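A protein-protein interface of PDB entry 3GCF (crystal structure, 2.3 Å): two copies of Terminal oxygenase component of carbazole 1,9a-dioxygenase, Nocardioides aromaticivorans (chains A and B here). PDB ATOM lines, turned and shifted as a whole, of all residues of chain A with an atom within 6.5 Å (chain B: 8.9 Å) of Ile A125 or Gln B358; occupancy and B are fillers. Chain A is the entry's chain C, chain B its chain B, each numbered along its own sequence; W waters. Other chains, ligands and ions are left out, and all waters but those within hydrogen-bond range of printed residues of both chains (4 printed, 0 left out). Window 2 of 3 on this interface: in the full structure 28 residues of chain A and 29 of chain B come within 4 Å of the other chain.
OH of Tyr B348 sits at hydrogen-bond distance from NE of Arg A78 (3.5 Å). N of Gln B358 is in hydrogen-bond range of O of Ala A76 (3.3 Å). N of Gln B358 sits at hydrogen-bond distance from O of His A77 (3.1 Å). OD2 of Asp B363 lies within hydrogen-bond range of NE2 of His A77 (2.7 Å).
The backbone carbonyl oxygen (O) of Phe B347 lies within hydrogen-bond range of the backbone NH (N) of Gly B353 (2.8 Å). The side-chain hydroxyl of Tyr B348 is in hydrogen-bond range of the side-chain carboxylate of Glu B357 (2.7 Å). NH2 of Arg B370 lies within salt-bridge range of OE2 of Glu B357, 2.4 Å away. N of Phe B360 sits at hydrogen-bond distance from OD2 of Asp B363 (3.0 Å). The backbone NH (N) of Ala A76 sits at hydrogen-bond distance from the side-chain hydroxyl (OH) of Tyr A103 (3.0 Å). O of Ile A125 is in hydrogen-bond range of N of Leu A110, 2.7 Å away.
Among the printed residues, pairs that only touch across the chains: Trp A101 with Gln B358, Arg A78 with Phe B347, His A77 with Glu B357, Ile A125 with Gln B358, Val A121 with Phe B360, His A77 with Phe B360, Trp A101 with Phe B360 and Val A121 with Leu B359.
Of the printed residues of chain B, Arg A78 touches Phe B347 (3.2 Å) and Tyr B348 (3.5 Å). Of the printed residues of chain B, Trp A101 touches Gln B358 (3.1 Å) and Phe B360 (3.8 Å). No residue of chain B comes within 4 Å of Arg A109. Ile A125 touches just one residue of chain B: Gln B358 (3.5 Å). Gly A126 touches none of the printed residues of chain B. Printed residues of chain A within 4 Å of Phe B347: Arg A78 (3.2 Å). Of the printed residues of chain A, Tyr B348 touches Arg A78. Ser B355 touches none of the printed residues of chain A. Of the printed residues of chain A, Gln B358 touches Ala A76, His A77, Trp A101 and Ile A125. Printed residues of chain A within 4 Å of Phe B360: His A77, Trp A101 and Val A121. The nearest residue of chain B that does not touch Ile A125 is Leu B359 (5.1 Å). The nearest residue of chain A that does not touch Gln B358 is Gly A126 (4.9 Å).
Of the 14 printed residues of chain B, 7 touch a printed residue of chain A. Printed residues of chain B that touch a printed residue of chain A: Phe B347, Tyr B348, Glu B357, Gln B358, Leu B359, Phe B360 and Asp B363. Hydrophobic or aromatic side chains of chain B within 4 Å of the printed part of chain A: Phe B347, Tyr B348 and Phe B360. Of the 16 printed residues of chain A, 6 touch a printed residue of chain B. Printed residues of chain A that touch a printed residue of chain B: Ala A76, His A77, Arg A78, Trp A101, Val A121 and Ile A125. Hydrophobic or aromatic side chains of chain A that line the printed part of chain B: Ala A76, His A77, Trp A101, Val A121 and Ile A125. Among the printed residues, no Asp or Glu carboxylate lies within 4 Å of a Lys or Arg side-chain nitrogen of the other chain.
No position is printed for both chains. Of the 12 pairs that touch across the chains among the printed residues, none has its exchanged pair printed and touching as well.
Water W1 lies within hydrogen-bond range of O of Lys B356 (2.6 Å), O of Ala A76 (2.8 Å) and NE2 of Gln B358 (3.3 Å). Water W3 bridges the backbone carbonyl oxygen of Gly A126 (2.7 Å) and the side-chain amide nitrogen of Gln B358 (2.9 Å). Water W2 bridges OD1 of Asp B363 and NH1 of Arg A78. Water W4 bridges the side-chain amide oxygen of Gln B358 (3.1 Å) and the backbone NH of Gly A126 (3.1 Å).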
ATOM      1  N   ALA A  76     -22.805  11.170  -8.868  1.00  0.00           N
ATOM      2  CA  ALA A  76     -23.342  10.458 -10.023  1.00  0.00           C
ATOM      3  C   ALA A  76     -24.006   9.141  -9.609  1.00  0.00           C
ATOM      4  O   ALA A  76     -24.876   8.632 -10.314  1.00  0.00           O
ATOM      5  CB  ALA A  76     -22.224  10.175 -11.027  1.00  0.00           C
ATOM      6  N   HIS A  77     -23.601   8.595  -8.466  1.00  0.00           N
ATOM      7  CA  HIS A  77     -24.140   7.320  -7.999  1.00  0.00           C
ATOM      8  C   HIS A  77     -25.630   7.381  -7.652  1.00  0.00           C
ATOM      9  O   HIS A  77     -26.473   6.939  -8.430  1.00  0.00           O
ATOM     10  CB  HIS A  77     -23.345   6.830  -6.787  1.00  0.00           C
ATOM     11  CG  HIS A  77     -23.748   5.467  -6.311  1.00  0.00           C
ATOM     12  ND1 HIS A  77     -23.493   5.020  -5.031  1.00  0.00           N
ATOM     13  CD2 HIS A  77     -24.357   4.443  -6.953  1.00  0.00           C
ATOM     14  CE1 HIS A  77     -23.929   3.779  -4.906  1.00  0.00           C
ATOM     15  NE2 HIS A  77     -24.455   3.405  -6.058  1.00  0.00           N
ATOM     16  N   ARG A  78     -25.955   7.924  -6.482  1.00  0.00           N
ATOM     17  CA  ARG A  78     -27.350   8.021  -6.079  1.00  0.00           C
ATOM     18  C   ARG A  78     -27.802   9.469  -5.894  1.00  0.00           C
ATOM     19  O   ARG A  78     -28.744   9.753  -5.156  1.00  0.00           O
ATOM     20  CB  ARG A  78     -27.592   7.201  -4.808  1.00  0.00           C
ATOM     21  CG  ARG A  78     -27.323   5.702  -4.994  1.00  0.00           C
ATOM     22  CD  ARG A  78     -27.801   4.908  -3.783  1.00  0.00           C
ATOM     23  NE  ARG A  78     -29.253   4.990  -3.643  1.00  0.00           N
ATOM     24  CZ  ARG A  78     -30.086   3.976  -3.858  1.00  0.00           C
ATOM     25  NH1 ARG A  78     -29.613   2.786  -4.217  1.00  0.00           N
ATOM     26  NH2 ARG A  78     -31.394   4.157  -3.734  1.00  0.00           N
ATOM     27  N   TRP A 101     -17.391   7.313  -3.700  1.00  0.00           N
ATOM     28  CA  TRP A 101     -17.024   7.622  -5.079  1.00  0.00           C
ATOM     29  C   TRP A 101     -16.184   8.899  -5.009  1.00  0.00           C
ATOM     30  O   TRP A 101     -16.573   9.874  -4.363  1.00  0.00           O
ATOM     31  CB  TRP A 101     -18.272   7.829  -5.936  1.00  0.00           C
ATOM     32  CG  TRP A 101     -18.932   6.536  -6.345  1.00  0.00           C
ATOM     33  CD1 TRP A 101     -18.948   5.356  -5.644  1.00  0.00           C
ATOM     34  CD2 TRP A 101     -19.708   6.307  -7.528  1.00  0.00           C
ATOM     35  NE1 TRP A 101     -19.687   4.413  -6.318  1.00  0.00           N
ATOM     36  CE2 TRP A 101     -20.166   4.970  -7.477  1.00  0.00           C
ATOM     37  CE3 TRP A 101     -20.063   7.106  -8.628  1.00  0.00           C
ATOM     38  CZ2 TRP A 101     -20.964   4.412  -8.483  1.00  0.00           C
ATOM     39  CZ3 TRP A 101     -20.854   6.552  -9.625  1.00  0.00           C
ATOM     40  CH2 TRP A 101     -21.296   5.214  -9.546  1.00  0.00           C
ATOM     41  N   TYR A 103     -14.003  11.950  -7.070  1.00  0.00           N
ATOM     42  CA  TYR A 103     -13.874  12.647  -8.339  1.00  0.00           C
ATOM     43  C   TYR A 103     -12.693  13.600  -8.444  1.00  0.00           C
ATOM     44  O   TYR A 103     -12.288  14.228  -7.466  1.00  0.00           O
ATOM     45  CB  TYR A 103     -15.154  13.431  -8.633  1.00  0.00           C
ATOM     46  CG  TYR A 103     -16.424  12.614  -8.537  1.00  0.00           C
ATOM     47  CD1 TYR A 103     -16.972  12.285  -7.296  1.00  0.00           C
ATOM     48  CD2 TYR A 103     -17.075  12.168  -9.685  1.00  0.00           C
ATOM     49  CE1 TYR A 103     -18.142  11.536  -7.202  1.00  0.00           C
ATOM     50  CE2 TYR A 103     -18.247  11.418  -9.599  1.00  0.00           C
ATOM     51  CZ  TYR A 103     -18.774  11.109  -8.353  1.00  0.00           C
ATOM     52  OH  TYR A 103     -19.942  10.392  -8.260  1.00  0.00           O
ATOM     53  N   GLY A 108     -13.833  16.394 -13.348  1.00  0.00           N
ATOM     54  CA  GLY A 108     -15.057  15.800 -12.829  1.00  0.00           C
ATOM     55  C   GLY A 108     -15.226  14.301 -13.016  1.00  0.00           C
ATOM     56  O   GLY A 108     -16.280  13.738 -12.693  1.00  0.00           O
ATOM     57  N   ARG A 109     -14.191  13.648 -13.526  1.00  0.00           N
ATOM     58  CA  ARG A 109     -14.234  12.210 -13.757  1.00  0.00           C
ATOM     59  C   ARG A 109     -14.114  11.387 -12.478  1.00  0.00           C
ATOM     60  O   ARG A 109     -13.434  11.780 -11.531  1.00  0.00           O
ATOM     61  CB  ARG A 109     -13.105  11.806 -14.711  1.00  0.00           C
ATOM     62  CG  ARG A 109     -13.265  12.303 -16.146  1.00  0.00           C
ATOM     63  CD  ARG A 109     -13.713  11.168 -17.057  1.00  0.00           C
ATOM     64  NE  ARG A 109     -15.106  11.285 -17.468  1.00  0.00           N
ATOM     65  CZ  ARG A 109     -15.823  10.283 -17.965  1.00  0.00           C
ATOM     66  NH1 ARG A 109     -15.280   9.082 -18.107  1.00  0.00           N
ATOM     67  NH2 ARG A 109     -17.082  10.482 -18.323  1.00  0.00           N
ATOM     68  N   LEU A 110     -14.787  10.240 -12.457  1.00  0.00           N
ATOM     69  CA  LEU A 110     -14.710   9.329 -11.320  1.00  0.00           C
ATOM     70  C   LEU A 110     -13.332   8.661 -11.430  1.00  0.00           C
ATOM     71  O   LEU A 110     -13.062   7.957 -12.402  1.00  0.00           O
ATOM     72  CB  LEU A 110     -15.810   8.271 -11.424  1.00  0.00           C
ATOM     73  CG  LEU A 110     -15.841   7.211 -10.320  1.00  0.00           C
ATOM     74  CD1 LEU A 110     -16.149   7.881  -8.990  1.00  0.00           C
ATOM     75  CD2 LEU A 110     -16.888   6.155 -10.642  1.00  0.00           C
ATOM     76  N   VAL A 111     -12.456   8.888 -10.456  1.00  0.00           N
ATOM     77  CA  VAL A 111     -11.125   8.293 -10.512  1.00  0.00           C
ATOM     78  C   VAL A 111     -10.906   7.204  -9.482  1.00  0.00           C
ATOM     79  O   VAL A 111      -9.858   6.557  -9.465  1.00  0.00           O
ATOM     80  CB  VAL A 111     -10.008   9.351 -10.334  1.00  0.00           C
ATOM     81  CG1 VAL A 111      -9.974  10.285 -11.544  1.00  0.00           C
ATOM     82  CG2 VAL A 111     -10.230  10.139  -9.045  1.00  0.00           C
ATOM     83  N   VAL A 121     -16.411   0.773 -12.823  1.00  0.00           N
ATOM     84  CA  VAL A 121     -17.062   2.024 -13.225  1.00  0.00           C
ATOM     85  C   VAL A 121     -16.062   3.173 -13.239  1.00  0.00           C
ATOM     86  O   VAL A 121     -16.337   4.235 -13.797  1.00  0.00           O
ATOM     87  CB  VAL A 121     -18.238   2.424 -12.293  1.00  0.00           C
ATOM     88  CG1 VAL A 121     -19.391   1.450 -12.463  1.00  0.00           C
ATOM     89  CG2 VAL A 121     -17.770   2.483 -10.846  1.00  0.00           C
ATOM     90  N   ILE A 122     -14.905   2.959 -12.620  1.00  0.00           N
ATOM     91  CA  ILE A 122     -13.868   3.984 -12.565  1.00  0.00           C
ATOM     92  C   ILE A 122     -13.447   4.358 -13.979  1.00  0.00           C
ATOM     93  O   ILE A 122     -13.178   3.484 -14.803  1.00  0.00           O
ATOM     94  CB  ILE A 122     -12.644   3.481 -11.781  1.00  0.00           C
ATOM     95  CG1 ILE A 122     -13.009   3.347 -10.302  1.00  0.00           C
ATOM     96  CG2 ILE A 122     -11.469   4.433 -11.967  1.00  0.00           C
ATOM     97  CD1 ILE A 122     -11.974   2.613  -9.481  1.00  0.00           C
ATOM     98  N   GLY A 123     -13.405   5.656 -14.262  1.00  0.00           N
ATOM     99  CA  GLY A 123     -13.028   6.108 -15.590  1.00  0.00           C
ATOM    100  C   GLY A 123     -14.157   6.063 -16.609  1.00  0.00           C
ATOM    101  O   GLY A 123     -13.976   6.483 -17.751  1.00  0.00           O
ATOM    102  N   LYS A 124     -15.326   5.567 -16.210  1.00  0.00           N
ATOM    103  CA  LYS A 124     -16.463   5.484 -17.124  1.00  0.00           C
ATOM    104  C   LYS A 124     -17.585   6.428 -16.712  1.00  0.00           C
ATOM    105  O   LYS A 124     -18.643   6.467 -17.338  1.00  0.00           O
ATOM    106  CB  LYS A 124     -17.007   4.052 -17.165  1.00  0.00           C
ATOM    107  CG  LYS A 124     -16.008   3.005 -17.660  1.00  0.00           C
ATOM    108  CD  LYS A 124     -16.654   1.621 -17.717  1.00  0.00           C
ATOM    109  CE  LYS A 124     -15.703   0.559 -18.282  1.00  0.00           C
ATOM    110  NZ  LYS A 124     -14.508   0.314 -17.411  1.00  0.00           N
ATOM    111  N   ILE A 125     -17.345   7.199 -15.661  1.00  0.00           N
ATOM    112  CA  ILE A 125     -18.355   8.115 -15.156  1.00  0.00           C
ATOM    113  C   ILE A 125     -17.767   9.471 -14.786  1.00  0.00           C
ATOM    114  O   ILE A 125     -16.587   9.578 -14.425  1.00  0.00           O
ATOM    115  CB  ILE A 125     -19.047   7.504 -13.908  1.00  0.00           C
ATOM    116  CG1 ILE A 125     -19.878   6.288 -14.328  1.00  0.00           C
ATOM    117  CG2 ILE A 125     -19.904   8.550 -13.201  1.00  0.00           C
ATOM    118  CD1 ILE A 125     -20.660   5.654 -13.198  1.00  0.00           C
ATOM    119  N   GLY A 126     -18.596  10.506 -14.874  1.00  0.00           N
ATOM    120  CA  GLY A 126     -18.144  11.834 -14.516  1.00  0.00           C
ATOM    121  C   GLY A 126     -19.289  12.783 -14.220  1.00  0.00           C
ATOM    122  O   GLY A 126     -20.436  12.531 -14.589  1.00  0.00           O
ATOM    123  N   ILE A 127     -18.987  13.871 -13.526  1.00  0.00           N
ATOM    124  CA  ILE A 127     -19.998  14.870 -13.227  1.00  0.00           C
ATOM    125  C   ILE A 127     -19.460  16.196 -13.741  1.00  0.00           C
ATOM    126  O   ILE A 127     -18.287  16.294 -14.108  1.00  0.00           O
ATOM    127  CB  ILE A 127     -20.301  14.958 -11.712  1.00  0.00           C
ATOM    128  CG1 ILE A 127     -19.001  15.056 -10.913  1.00  0.00           C
ATOM    129  CG2 ILE A 127     -21.134  13.754 -11.280  1.00  0.00           C
ATOM    130  CD1 ILE A 127     -19.235  15.223  -9.426  1.00  0.00           C
ATOM    131  N   PHE B 347     -33.545  13.878  -5.177  1.00  0.00           N
ATOM    132  CA  PHE B 347     -33.085  13.235  -6.402  1.00  0.00           C
ATOM    133  C   PHE B 347     -34.070  12.199  -6.929  1.00  0.00           C
ATOM    134  O   PHE B 347     -34.498  12.276  -8.083  1.00  0.00           O
ATOM    135  CB  PHE B 347     -31.722  12.573  -6.169  1.00  0.00           C
ATOM    136  CG  PHE B 347     -31.147  11.902  -7.393  1.00  0.00           C
ATOM    137  CD1 PHE B 347     -30.859  12.641  -8.539  1.00  0.00           C
ATOM    138  CD2 PHE B 347     -30.854  10.540  -7.383  1.00  0.00           C
ATOM    139  CE1 PHE B 347     -30.281  12.035  -9.661  1.00  0.00           C
ATOM    140  CE2 PHE B 347     -30.276   9.919  -8.495  1.00  0.00           C
ATOM    141  CZ  PHE B 347     -29.988  10.671  -9.638  1.00  0.00           C
ATOM    142  N   TYR B 348     -34.420  11.226  -6.090  1.00  0.00           N
ATOM    143  CA  TYR B 348     -35.346  10.167  -6.492  1.00  0.00           C
ATOM    144  C   TYR B 348     -36.816  10.568  -6.453  1.00  0.00           C
ATOM    145  O   TYR B 348     -37.612  10.079  -7.248  1.00  0.00           O
ATOM    146  CB  TYR B 348     -35.165   8.921  -5.615  1.00  0.00           C
ATOM    147  CG  TYR B 348     -33.908   8.135  -5.902  1.00  0.00           C
ATOM    148  CD1 TYR B 348     -32.710   8.432  -5.250  1.00  0.00           C
ATOM    149  CD2 TYR B 348     -33.914   7.096  -6.836  1.00  0.00           C
ATOM    150  CE1 TYR B 348     -31.549   7.717  -5.518  1.00  0.00           C
ATOM    151  CE2 TYR B 348     -32.757   6.371  -7.113  1.00  0.00           C
ATOM    152  CZ  TYR B 348     -31.578   6.691  -6.449  1.00  0.00           C
ATOM    153  OH  TYR B 348     -30.428   5.995  -6.729  1.00  0.00           O
ATOM    154  N   GLY B 353     -34.706  10.407 -10.155  1.00  0.00           N
ATOM    155  CA  GLY B 353     -33.455   9.716  -9.914  1.00  0.00           C
ATOM    156  C   GLY B 353     -33.481   8.251 -10.310  1.00  0.00           C
ATOM    157  O   GLY B 353     -32.429   7.658 -10.536  1.00  0.00           O
ATOM    158  N   TRP B 354     -34.670   7.660 -10.403  1.00  0.00           N
ATOM    159  CA  TRP B 354     -34.772   6.250 -10.772  1.00  0.00           C
ATOM    160  C   TRP B 354     -34.226   5.988 -12.165  1.00  0.00           C
ATOM    161  O   TRP B 354     -33.758   4.886 -12.451  1.00  0.00           O
ATOM    162  CB  TRP B 354     -36.221   5.757 -10.693  1.00  0.00           C
ATOM    163  CG  TRP B 354     -36.813   5.848  -9.313  1.00  0.00           C
ATOM    164  CD1 TRP B 354     -37.773   6.719  -8.891  1.00  0.00           C
ATOM    165  CD2 TRP B 354     -36.453   5.065  -8.168  1.00  0.00           C
ATOM    166  NE1 TRP B 354     -38.032   6.532  -7.556  1.00  0.00           N
ATOM    167  CE2 TRP B 354     -37.237   5.522  -7.086  1.00  0.00           C
ATOM    168  CE3 TRP B 354     -35.543   4.022  -7.950  1.00  0.00           C
ATOM    169  CZ2 TRP B 354     -37.139   4.973  -5.801  1.00  0.00           C
ATOM    170  CZ3 TRP B 354     -35.443   3.477  -6.672  1.00  0.00           C
ATOM    171  CH2 TRP B 354     -36.239   3.956  -5.615  1.00  0.00           C
ATOM    172  N   SER B 355     -34.270   6.990 -13.038  1.00  0.00           N
ATOM    173  CA  SER B 355     -33.749   6.784 -14.384  1.00  0.00           C
ATOM    174  C   SER B 355     -32.405   7.472 -14.612  1.00  0.00           C
ATOM    175  O   SER B 355     -31.817   7.334 -15.678  1.00  0.00           O
ATOM    176  CB  SER B 355     -34.756   7.264 -15.437  1.00  0.00           C
ATOM    177  OG  SER B 355     -34.799   8.678 -15.507  1.00  0.00           O
ATOM    178  N   LYS B 356     -31.907   8.197 -13.616  1.00  0.00           N
ATOM    179  CA  LYS B 356     -30.636   8.896 -13.774  1.00  0.00           C
ATOM    180  C   LYS B 356     -29.494   8.342 -12.926  1.00  0.00           C
ATOM    181  O   LYS B 356     -28.327   8.623 -13.188  1.00  0.00           O
ATOM    182  CB  LYS B 356     -30.824  10.385 -13.481  1.00  0.00           C
ATOM    183  CG  LYS B 356     -31.792  11.063 -14.432  1.00  0.00           C
ATOM    184  CD  LYS B 356     -31.949  12.541 -14.122  1.00  0.00           C
ATOM    185  CE  LYS B 356     -32.916  13.196 -15.105  1.00  0.00           C
ATOM    186  NZ  LYS B 356     -32.520  12.951 -16.532  1.00  0.00           N
ATOM    187  N   GLU B 357     -29.833   7.562 -11.908  1.00  0.00           N
ATOM    188  CA  GLU B 357     -28.830   6.958 -11.045  1.00  0.00           C
ATOM    189  C   GLU B 357     -27.839   6.173 -11.898  1.00  0.00           C
ATOM    190  O   GLU B 357     -28.173   5.716 -12.990  1.00  0.00           O
ATOM    191  CB  GLU B 357     -29.498   5.995 -10.058  1.00  0.00           C
ATOM    192  CG  GLU B 357     -30.367   4.947 -10.751  1.00  0.00           C
ATOM    193  CD  GLU B 357     -30.873   3.860  -9.818  1.00  0.00           C
ATOM    194  OE1 GLU B 357     -30.981   4.104  -8.595  1.00  0.00           O
ATOM    195  OE2 GLU B 357     -31.178   2.759 -10.317  1.00  0.00           O
ATOM    196  N   GLN B 358     -26.619   6.026 -11.405  1.00  0.00           N
ATOM    197  CA  GLN B 358     -25.604   5.257 -12.115  1.00  0.00           C
ATOM    198  C   GLN B 358     -25.050   4.291 -11.077  1.00  0.00           C
ATOM    199  O   GLN B 358     -24.271   4.673 -10.205  1.00  0.00           O
ATOM    200  CB  GLN B 358     -24.518   6.182 -12.680  1.00  0.00           C
ATOM    201  CG  GLN B 358     -25.068   7.169 -13.712  1.00  0.00           C
ATOM    202  CD  GLN B 358     -23.997   8.022 -14.365  1.00  0.00           C
ATOM    203  OE1 GLN B 358     -23.110   7.511 -15.047  1.00  0.00           O
ATOM    204  NE2 GLN B 358     -24.077   9.335 -14.163  1.00  0.00           N
ATOM    205  N   LEU B 359     -25.489   3.041 -11.164  1.00  0.00           N
ATOM    206  CA  LEU B 359     -25.084   2.014 -10.209  1.00  0.00           C
ATOM    207  C   LEU B 359     -23.753   1.344 -10.524  1.00  0.00           C
ATOM    208  O   LEU B 359     -23.176   1.559 -11.588  1.00  0.00           O
ATOM    209  CB  LEU B 359     -26.179   0.951 -10.119  1.00  0.00           C
ATOM    210  CG  LEU B 359     -27.584   1.506  -9.856  1.00  0.00           C
ATOM    211  CD1 LEU B 359     -28.600   0.372  -9.813  1.00  0.00           C
ATOM    212  CD2 LEU B 359     -27.588   2.275  -8.543  1.00  0.00           C
ATOM    213  N   PHE B 360     -23.249   0.566  -9.571  1.00  0.00           N
ATOM    214  CA  PHE B 360     -22.017  -0.175  -9.778  1.00  0.00           C
ATOM    215  C   PHE B 360     -22.205  -1.588  -9.213  1.00  0.00           C
ATOM    216  O   PHE B 360     -23.150  -1.836  -8.468  1.00  0.00           O
ATOM    217  CB  PHE B 360     -20.787   0.601  -9.230  1.00  0.00           C
ATOM    218  CG  PHE B 360     -20.643   0.630  -7.727  1.00  0.00           C
ATOM    219  CD1 PHE B 360     -21.692   1.008  -6.902  1.00  0.00           C
ATOM    220  CD2 PHE B 360     -19.397   0.367  -7.149  1.00  0.00           C
ATOM    221  CE1 PHE B 360     -21.504   1.132  -5.518  1.00  0.00           C
ATOM    222  CE2 PHE B 360     -19.196   0.486  -5.768  1.00  0.00           C
ATOM    223  CZ  PHE B 360     -20.251   0.870  -4.955  1.00  0.00           C
ATOM    224  N   PRO B 361     -21.329  -2.540  -9.582  1.00  0.00           N
ATOM    225  CA  PRO B 361     -21.423  -3.932  -9.127  1.00  0.00           C
ATOM    226  C   PRO B 361     -22.091  -4.288  -7.797  1.00  0.00           C
ATOM    227  O   PRO B 361     -23.000  -5.116  -7.772  1.00  0.00           O
ATOM    228  CB  PRO B 361     -19.983  -4.423  -9.236  1.00  0.00           C
ATOM    229  CG  PRO B 361     -19.541  -3.743 -10.509  1.00  0.00           C
ATOM    230  CD  PRO B 361     -20.067  -2.320 -10.317  1.00  0.00           C
ATOM    231  N   ASP B 363     -24.287  -2.830  -6.179  1.00  0.00           N
ATOM    232  CA  ASP B 363     -25.717  -2.519  -6.188  1.00  0.00           C
ATOM    233  C   ASP B 363     -26.584  -3.604  -6.814  1.00  0.00           C
ATOM    234  O   ASP B 363     -27.811  -3.514  -6.770  1.00  0.00           O
ATOM    235  CB  ASP B 363     -25.992  -1.198  -6.917  1.00  0.00           C
ATOM    236  CG  ASP B 363     -25.301  -0.016  -6.269  1.00  0.00           C
ATOM    237  OD1 ASP B 363     -25.259   0.041  -5.021  1.00  0.00           O
ATOM    238  OD2 ASP B 363     -24.810   0.860  -7.013  1.00  0.00           O
ATOM    239  N   MET B 364     -25.967  -4.628  -7.396  1.00  0.00           N
ATOM    240  CA  MET B 364     -26.751  -5.685  -8.021  1.00  0.00           C
ATOM    241  C   MET B 364     -27.716  -6.369  -7.065  1.00  0.00           C
ATOM    242  O   MET B 364     -28.768  -6.839  -7.486  1.00  0.00           O
ATOM    243  CB  MET B 364     -25.844  -6.729  -8.674  1.00  0.00           C
ATOM    244  CG  MET B 364     -25.160  -6.221  -9.936  1.00  0.00           C
ATOM    245  SD  MET B 364     -26.334  -5.496 -11.130  1.00  0.00           S
ATOM    246  CE  MET B 364     -25.937  -3.706 -10.977  1.00  0.00           C
ATOM    247  N   ARG B 370     -35.292  -5.159  -6.464  1.00  0.00           N
ATOM    248  CA  ARG B 370     -36.287  -4.361  -7.175  1.00  0.00           C
ATOM    249  C   ARG B 370     -37.021  -5.224  -8.190  1.00  0.00           C
ATOM    250  O   ARG B 370     -38.229  -5.086  -8.379  1.00  0.00           O
ATOM    251  CB  ARG B 370     -35.614  -3.152  -7.843  1.00  0.00           C
ATOM    252  CG  ARG B 370     -34.635  -2.469  -6.893  1.00  0.00           C
ATOM    253  CD  ARG B 370     -34.527  -0.949  -7.007  1.00  0.00           C
ATOM    254  NE  ARG B 370     -33.786  -0.492  -8.168  1.00  0.00           N
ATOM    255  CZ  ARG B 370     -33.028   0.605  -8.191  1.00  0.00           C
ATOM    256  NH1 ARG B 370     -32.898   1.363  -7.110  1.00  0.00           N
ATOM    257  NH2 ARG B 370     -32.418   0.957  -9.311  1.00  0.00           N
HETATM  258  O   HOH W   1     -26.493  10.103 -12.041  1.00  0.00           O
HETATM  259  O   HOH W   2     -26.871   1.932  -3.567  1.00  0.00           O
HETATM  260  O   HOH W   3     -23.084  12.048 -14.330  1.00  0.00           O
HETATM  261  O   HOH W   4     -21.358   9.762 -16.168  1.00  0.00           O
